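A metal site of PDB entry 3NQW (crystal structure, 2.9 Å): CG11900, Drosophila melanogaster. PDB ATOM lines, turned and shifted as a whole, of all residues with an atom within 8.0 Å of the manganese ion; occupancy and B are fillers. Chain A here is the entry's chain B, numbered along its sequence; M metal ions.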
ATOM      1  N   HIS A  20      -0.744 -27.077   2.124  1.00  0.00           N
ATOM      2  CA  HIS A  20      -2.072 -26.649   2.573  1.00  0.00           C
ATOM      3  C   HIS A  20      -2.186 -26.898   4.063  1.00  0.00           C
ATOM      4  O   HIS A  20      -3.205 -26.593   4.645  1.00  0.00           O
ATOM      5  CB  HIS A  20      -3.183 -27.465   1.905  1.00  0.00           C
ATOM      6  CG  HIS A  20      -3.460 -27.109   0.481  1.00  0.00           C
ATOM      7  ND1 HIS A  20      -4.021 -25.893   0.116  1.00  0.00           N
ATOM      8  CD2 HIS A  20      -3.366 -27.822  -0.657  1.00  0.00           C
ATOM      9  CE1 HIS A  20      -4.264 -25.897  -1.176  1.00  0.00           C
ATOM     10  NE2 HIS A  20      -3.865 -27.060  -1.678  1.00  0.00           N
ATOM     11  N   GLN A  23      -4.265 -24.406   5.866  1.00  0.00           N
ATOM     12  CA  GLN A  23      -5.530 -24.015   5.257  1.00  0.00           C
ATOM     13  C   GLN A  23      -6.652 -24.971   5.620  1.00  0.00           C
ATOM     14  O   GLN A  23      -6.448 -26.188   5.632  1.00  0.00           O
ATOM     15  CB  GLN A  23      -5.371 -23.960   3.737  1.00  0.00           C
ATOM     16  CG  GLN A  23      -6.587 -23.511   2.952  1.00  0.00           C
ATOM     17  CD  GLN A  23      -6.306 -23.452   1.467  1.00  0.00           C
ATOM     18  OE1 GLN A  23      -7.219 -23.407   0.648  1.00  0.00           O
ATOM     19  NE2 GLN A  23      -5.023 -23.438   1.105  1.00  0.00           N
ATOM     20  N   TYR A  33      -8.193 -28.292   4.639  1.00  0.00           N
ATOM     21  CA  TYR A  33      -8.501 -28.006   3.247  1.00  0.00           C
ATOM     22  C   TYR A  33      -7.963 -29.090   2.326  1.00  0.00           C
ATOM     23  O   TYR A  33      -8.461 -29.284   1.224  1.00  0.00           O
ATOM     24  CB  TYR A  33      -7.959 -26.629   2.836  1.00  0.00           C
ATOM     25  CG  TYR A  33      -8.542 -26.140   1.523  1.00  0.00           C
ATOM     26  CD1 TYR A  33      -8.018 -26.572   0.308  1.00  0.00           C
ATOM     27  CD2 TYR A  33      -9.620 -25.251   1.493  1.00  0.00           C
ATOM     28  CE1 TYR A  33      -8.544 -26.144  -0.903  1.00  0.00           C
ATOM     29  CE2 TYR A  33     -10.164 -24.805   0.281  1.00  0.00           C
ATOM     30  CZ  TYR A  33      -9.614 -25.262  -0.914  1.00  0.00           C
ATOM     31  OH  TYR A  33     -10.110 -24.832  -2.128  1.00  0.00           O
ATOM     32  N   HIS A  36     -10.458 -31.347   0.686  1.00  0.00           N
ATOM     33  CA  HIS A  36     -11.024 -30.896  -0.565  1.00  0.00           C
ATOM     34  C   HIS A  36     -10.259 -31.405  -1.781  1.00  0.00           C
ATOM     35  O   HIS A  36     -10.788 -32.195  -2.563  1.00  0.00           O
ATOM     36  CB  HIS A  36     -11.015 -29.372  -0.610  1.00  0.00           C
ATOM     37  CG  HIS A  36     -11.478 -28.819  -1.918  1.00  0.00           C
ATOM     38  ND1 HIS A  36     -12.706 -29.143  -2.456  1.00  0.00           N
ATOM     39  CD2 HIS A  36     -10.878 -28.001  -2.811  1.00  0.00           C
ATOM     40  CE1 HIS A  36     -12.842 -28.538  -3.630  1.00  0.00           C
ATOM     41  NE2 HIS A  36     -11.753 -27.841  -3.866  1.00  0.00           N
ATOM     42  N   VAL A  37      -9.008 -30.942  -1.940  1.00  0.00           N
ATOM     43  CA  VAL A  37      -8.178 -31.292  -3.084  1.00  0.00           C
ATOM     44  C   VAL A  37      -8.210 -32.774  -3.349  1.00  0.00           C
ATOM     45  O   VAL A  37      -8.363 -33.192  -4.493  1.00  0.00           O
ATOM     46  CB  VAL A  37      -6.727 -30.740  -2.943  1.00  0.00           C
ATOM     47  CG1 VAL A  37      -6.761 -29.230  -2.882  1.00  0.00           C
ATOM     48  CG2 VAL A  37      -6.048 -31.310  -1.728  1.00  0.00           C
ATOM     49  N   VAL A  40     -11.471 -33.848  -4.643  1.00  0.00           N
ATOM     50  CA  VAL A  40     -11.416 -33.451  -6.061  1.00  0.00           C
ATOM     51  C   VAL A  40     -10.613 -34.437  -6.916  1.00  0.00           C
ATOM     52  O   VAL A  40     -11.070 -34.925  -7.960  1.00  0.00           O
ATOM     53  CB  VAL A  40     -10.806 -32.022  -6.235  1.00  0.00           C
ATOM     54  CG1 VAL A  40     -10.523 -31.735  -7.733  1.00  0.00           C
ATOM     55  CG2 VAL A  40     -11.772 -30.989  -5.675  1.00  0.00           C
ATOM     56  N   ALA A  59      -4.953 -32.293 -10.178  1.00  0.00           N
ATOM     57  CA  ALA A  59      -6.090 -32.068  -9.283  1.00  0.00           C
ATOM     58  C   ALA A  59      -5.615 -31.938  -7.840  1.00  0.00           C
ATOM     59  O   ALA A  59      -6.168 -31.156  -7.068  1.00  0.00           O
ATOM     60  CB  ALA A  59      -7.088 -33.207  -9.404  1.00  0.00           C
ATOM     61  N   HIS A  62      -4.710 -28.405  -7.657  1.00  0.00           N
ATOM     62  CA  HIS A  62      -5.627 -27.470  -8.270  1.00  0.00           C
ATOM     63  C   HIS A  62      -6.020 -26.293  -7.378  1.00  0.00           C
ATOM     64  O   HIS A  62      -7.063 -25.685  -7.595  1.00  0.00           O
ATOM     65  CB  HIS A  62      -6.895 -28.196  -8.712  1.00  0.00           C
ATOM     66  CG  HIS A  62      -7.972 -28.252  -7.686  1.00  0.00           C
ATOM     67  ND1 HIS A  62      -7.886 -29.038  -6.546  1.00  0.00           N
ATOM     68  CD2 HIS A  62      -9.181 -27.647  -7.616  1.00  0.00           C
ATOM     69  CE1 HIS A  62      -8.983 -28.910  -5.848  1.00  0.00           C
ATOM     70  NE2 HIS A  62      -9.791 -28.056  -6.466  1.00  0.00           N
ATOM     71  N   ASP A  63      -5.218 -25.987  -6.366  1.00  0.00           N
ATOM     72  CA  ASP A  63      -5.511 -24.844  -5.489  1.00  0.00           C
ATOM     73  C   ASP A  63      -4.260 -24.370  -4.751  1.00  0.00           C
ATOM     74  O   ASP A  63      -4.324 -23.364  -4.048  1.00  0.00           O
ATOM     75  CB  ASP A  63      -6.635 -25.164  -4.465  1.00  0.00           C
ATOM     76  CG  ASP A  63      -8.063 -24.876  -5.009  1.00  0.00           C
ATOM     77  OD1 ASP A  63      -8.308 -23.798  -5.597  1.00  0.00           O
ATOM     78  OD2 ASP A  63      -8.952 -25.744  -4.819  1.00  0.00           O
ATOM     79  N   VAL A  64      -3.129 -25.059  -4.917  1.00  0.00           N
ATOM     80  CA  VAL A  64      -1.892 -24.655  -4.245  1.00  0.00           C
ATOM     81  C   VAL A  64      -1.332 -23.340  -4.761  1.00  0.00           C
ATOM     82  O   VAL A  64      -1.158 -22.386  -4.001  1.00  0.00           O
ATOM     83  CB  VAL A  64      -0.747 -25.684  -4.404  1.00  0.00           C
ATOM     84  CG1 VAL A  64      -0.981 -26.870  -3.517  1.00  0.00           C
ATOM     85  CG2 VAL A  64      -0.612 -26.086  -5.850  1.00  0.00           C
ATOM     86  N   GLU A  66      -2.691 -21.209  -6.104  1.00  0.00           N
ATOM     87  CA  GLU A  66      -3.715 -20.186  -5.971  1.00  0.00           C
ATOM     88  C   GLU A  66      -4.027 -19.818  -4.523  1.00  0.00           C
ATOM     89  O   GLU A  66      -4.216 -18.651  -4.219  1.00  0.00           O
ATOM     90  CB  GLU A  66      -4.991 -20.632  -6.691  1.00  0.00           C
ATOM     91  CG  GLU A  66      -5.816 -19.497  -7.279  1.00  0.00           C
ATOM     92  CD  GLU A  66      -7.318 -19.762  -7.244  1.00  0.00           C
ATOM     93  OE1 GLU A  66      -8.021 -19.001  -6.535  1.00  0.00           O
ATOM     94  OE2 GLU A  66      -7.775 -20.718  -7.905  1.00  0.00           O
ATOM     95  N   ASP A  67      -4.086 -20.798  -3.627  1.00  0.00           N
ATOM     96  CA  ASP A  67      -4.394 -20.476  -2.234  1.00  0.00           C
ATOM     97  C   ASP A  67      -3.181 -20.625  -1.312  1.00  0.00           C
ATOM     98  O   ASP A  67      -3.252 -20.351  -0.118  1.00  0.00           O
ATOM     99  CB  ASP A  67      -5.546 -21.361  -1.725  1.00  0.00           C
ATOM    100  CG  ASP A  67      -6.773 -21.318  -2.625  1.00  0.00           C
ATOM    101  OD1 ASP A  67      -7.340 -20.205  -2.830  1.00  0.00           O
ATOM    102  OD2 ASP A  67      -7.166 -22.388  -3.139  1.00  0.00           O
ATOM    103  N   VAL A  90      -5.949 -24.206 -14.555  1.00  0.00           N
ATOM    104  CA  VAL A  90      -7.047 -24.196 -13.620  1.00  0.00           C
ATOM    105  C   VAL A  90      -6.847 -23.236 -12.466  1.00  0.00           C
ATOM    106  O   VAL A  90      -7.631 -23.221 -11.524  1.00  0.00           O
ATOM    107  CB  VAL A  90      -7.339 -25.610 -13.085  1.00  0.00           C
ATOM    108  CG1 VAL A  90      -7.768 -26.511 -14.228  1.00  0.00           C
ATOM    109  CG2 VAL A  90      -6.099 -26.164 -12.422  1.00  0.00           C
ATOM    110  N   ILE A 119     -10.822 -31.365 -14.397  1.00  0.00           N
ATOM    111  CA  ILE A 119     -10.467 -30.834 -13.086  1.00  0.00           C
ATOM    112  C   ILE A 119     -11.464 -29.753 -12.672  1.00  0.00           C
ATOM    113  O   ILE A 119     -11.941 -29.731 -11.544  1.00  0.00           O
ATOM    114  CB  ILE A 119      -9.039 -30.202 -13.099  1.00  0.00           C
ATOM    115  CG1 ILE A 119      -8.004 -31.276 -13.451  1.00  0.00           C
ATOM    116  CG2 ILE A 119      -8.737 -29.537 -11.772  1.00  0.00           C
ATOM    117  CD1 ILE A 119      -6.590 -30.755 -13.538  1.00  0.00           C
ATOM    118  N   LYS A 120     -11.791 -28.863 -13.607  1.00  0.00           N
ATOM    119  CA  LYS A 120     -12.718 -27.790 -13.352  1.00  0.00           C
ATOM    120  C   LYS A 120     -14.077 -28.288 -12.900  1.00  0.00           C
ATOM    121  O   LYS A 120     -14.638 -27.739 -11.961  1.00  0.00           O
ATOM    122  CB  LYS A 120     -12.871 -26.949 -14.601  1.00  0.00           C
ATOM    123  CG  LYS A 120     -11.552 -26.427 -15.166  1.00  0.00           C
ATOM    124  CD  LYS A 120     -11.660 -24.934 -15.457  1.00  0.00           C
ATOM    125  CE  LYS A 120     -10.542 -24.486 -16.348  1.00  0.00           C
ATOM    126  NZ  LYS A 120     -10.590 -23.018 -16.500  1.00  0.00           N
ATOM    127  N   ALA A 122     -14.791 -31.300 -11.568  1.00  0.00           N
ATOM    128  CA  ALA A 122     -14.592 -31.947 -10.288  1.00  0.00           C
ATOM    129  C   ALA A 122     -14.551 -30.878  -9.189  1.00  0.00           C
ATOM    130  O   ALA A 122     -15.290 -30.961  -8.209  1.00  0.00           O
ATOM    131  CB  ALA A 122     -13.298 -32.735 -10.288  1.00  0.00           C
ATOM    132  N   ASP A 123     -13.705 -29.867  -9.369  1.00  0.00           N
ATOM    133  CA  ASP A 123     -13.579 -28.783  -8.396  1.00  0.00           C
ATOM    134  C   ASP A 123     -14.971 -28.275  -8.081  1.00  0.00           C
ATOM    135  O   ASP A 123     -15.307 -28.017  -6.933  1.00  0.00           O
ATOM    136  CB  ASP A 123     -12.734 -27.640  -8.948  1.00  0.00           C
ATOM    137  CG  ASP A 123     -12.365 -26.618  -7.877  1.00  0.00           C
ATOM    138  OD1 ASP A 123     -12.024 -25.466  -8.253  1.00  0.00           O
ATOM    139  OD2 ASP A 123     -12.408 -26.949  -6.673  1.00  0.00           O
ATOM    140  N   LYS A 124     -15.782 -28.121  -9.116  1.00  0.00           N
ATOM    141  CA  LYS A 124     -17.126 -27.634  -8.901  1.00  0.00           C
ATOM    142  C   LYS A 124     -17.962 -28.664  -8.156  1.00  0.00           C
ATOM    143  O   LYS A 124     -18.456 -28.394  -7.056  1.00  0.00           O
ATOM    144  CB  LYS A 124     -17.795 -27.262 -10.229  1.00  0.00           C
ATOM    145  CG  LYS A 124     -17.276 -25.945 -10.797  1.00  0.00           C
ATOM    146  CD  LYS A 124     -17.574 -24.775  -9.876  1.00  0.00           C
ATOM    147  CE  LYS A 124     -16.755 -23.572 -10.293  1.00  0.00           C
ATOM    148  NZ  LYS A 124     -15.295 -23.976 -10.301  1.00  0.00           N
ATOM    149  N   ASP A 126     -17.365 -31.292  -6.306  1.00  0.00           N
ATOM    150  CA  ASP A 126     -16.990 -31.440  -4.913  1.00  0.00           C
ATOM    151  C   ASP A 126     -17.416 -30.230  -4.082  1.00  0.00           C
ATOM    152  O   ASP A 126     -17.976 -30.383  -3.012  1.00  0.00           O
ATOM    153  CB  ASP A 126     -15.476 -31.673  -4.787  1.00  0.00           C
ATOM    154  CG  ASP A 126     -15.031 -31.801  -3.348  1.00  0.00           C
ATOM    155  OD1 ASP A 126     -15.607 -32.632  -2.609  1.00  0.00           O
ATOM    156  OD2 ASP A 126     -14.082 -31.092  -2.953  1.00  0.00           O
ATOM    157  N   ASN A 127     -17.145 -29.033  -4.569  1.00  0.00           N
ATOM    158  CA  ASN A 127     -17.543 -27.866  -3.788  1.00  0.00           C
ATOM    159  C   ASN A 127     -19.026 -27.879  -3.514  1.00  0.00           C
ATOM    160  O   ASN A 127     -19.456 -27.692  -2.377  1.00  0.00           O
ATOM    161  CB  ASN A 127     -17.168 -26.569  -4.501  1.00  0.00           C
ATOM    162  CG  ASN A 127     -15.695 -26.249  -4.366  1.00  0.00           C
ATOM    163  OD1 ASN A 127     -15.162 -26.188  -3.255  1.00  0.00           O
ATOM    164  ND2 ASN A 127     -15.018 -26.052  -5.493  1.00  0.00           N
ATOM    165  N   TYR A 147     -23.888 -18.756  -5.395  1.00  0.00           N
ATOM    166  CA  TYR A 147     -22.802 -19.640  -5.761  1.00  0.00           C
ATOM    167  C   TYR A 147     -23.324 -20.678  -6.740  1.00  0.00           C
ATOM    168  O   TYR A 147     -22.675 -20.956  -7.747  1.00  0.00           O
ATOM    169  CB  TYR A 147     -22.221 -20.369  -4.554  1.00  0.00           C
ATOM    170  CG  TYR A 147     -20.897 -21.048  -4.856  1.00  0.00           C
ATOM    171  CD1 TYR A 147     -19.694 -20.393  -4.611  1.00  0.00           C
ATOM    172  CD2 TYR A 147     -20.845 -22.315  -5.405  1.00  0.00           C
ATOM    173  CE1 TYR A 147     -18.462 -20.993  -4.933  1.00  0.00           C
ATOM    174  CE2 TYR A 147     -19.624 -22.921  -5.734  1.00  0.00           C
ATOM    175  CZ  TYR A 147     -18.442 -22.257  -5.492  1.00  0.00           C
ATOM    176  OH  TYR A 147     -17.237 -22.849  -5.807  1.00  0.00           O
HETATM  177 MN    MN M   1     -10.971 -26.073  -5.253  1.00  0.00          MN
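The side-chain amide nitrogen (ND2) of Asn 127 lies within hydrogen-bond range of the backbone carbonyl oxygen (O) of Asp 123 (2.5 Å).
A ring nitrogen (ND1) of His 62 sits at hydrogen-bond distance from the backbone carbonyl oxygen (O) of Ala 59 (2.8 Å).
The side-chain hydroxyl (OH) of Tyr 33 lies close to the side-chain carboxylate (OD2) of Asp 63.
The backbone NH (N) of Tyr 33 sits at hydrogen-bond distance from the backbone carbonyl oxygen (O) of Gln 23 (2.9 Å).
ND1 of His 36 sits at hydrogen-bond distance from OD2 of Asp 126 (2.4 Å).
The manganese ion is bound by the side-chain carboxylate (OD2) of Asp 63, the side-chain carboxylate (OD2) of Asp 123, a ring nitrogen (NE2) of His 36 and a ring nitrogen (NE2) of His 62.
The manganese ion has four donor atoms within binding distance.
Tyr 33 touches the manganese ion (OH to MN, 3.5 Å).
Within 4 Å of the manganese ion: Tyr 33, His 36, His 62, Asp 63 and Asp 123.
The nearest printed residue that does not touch the manganese ion is Asn 127 (4.1 Å).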
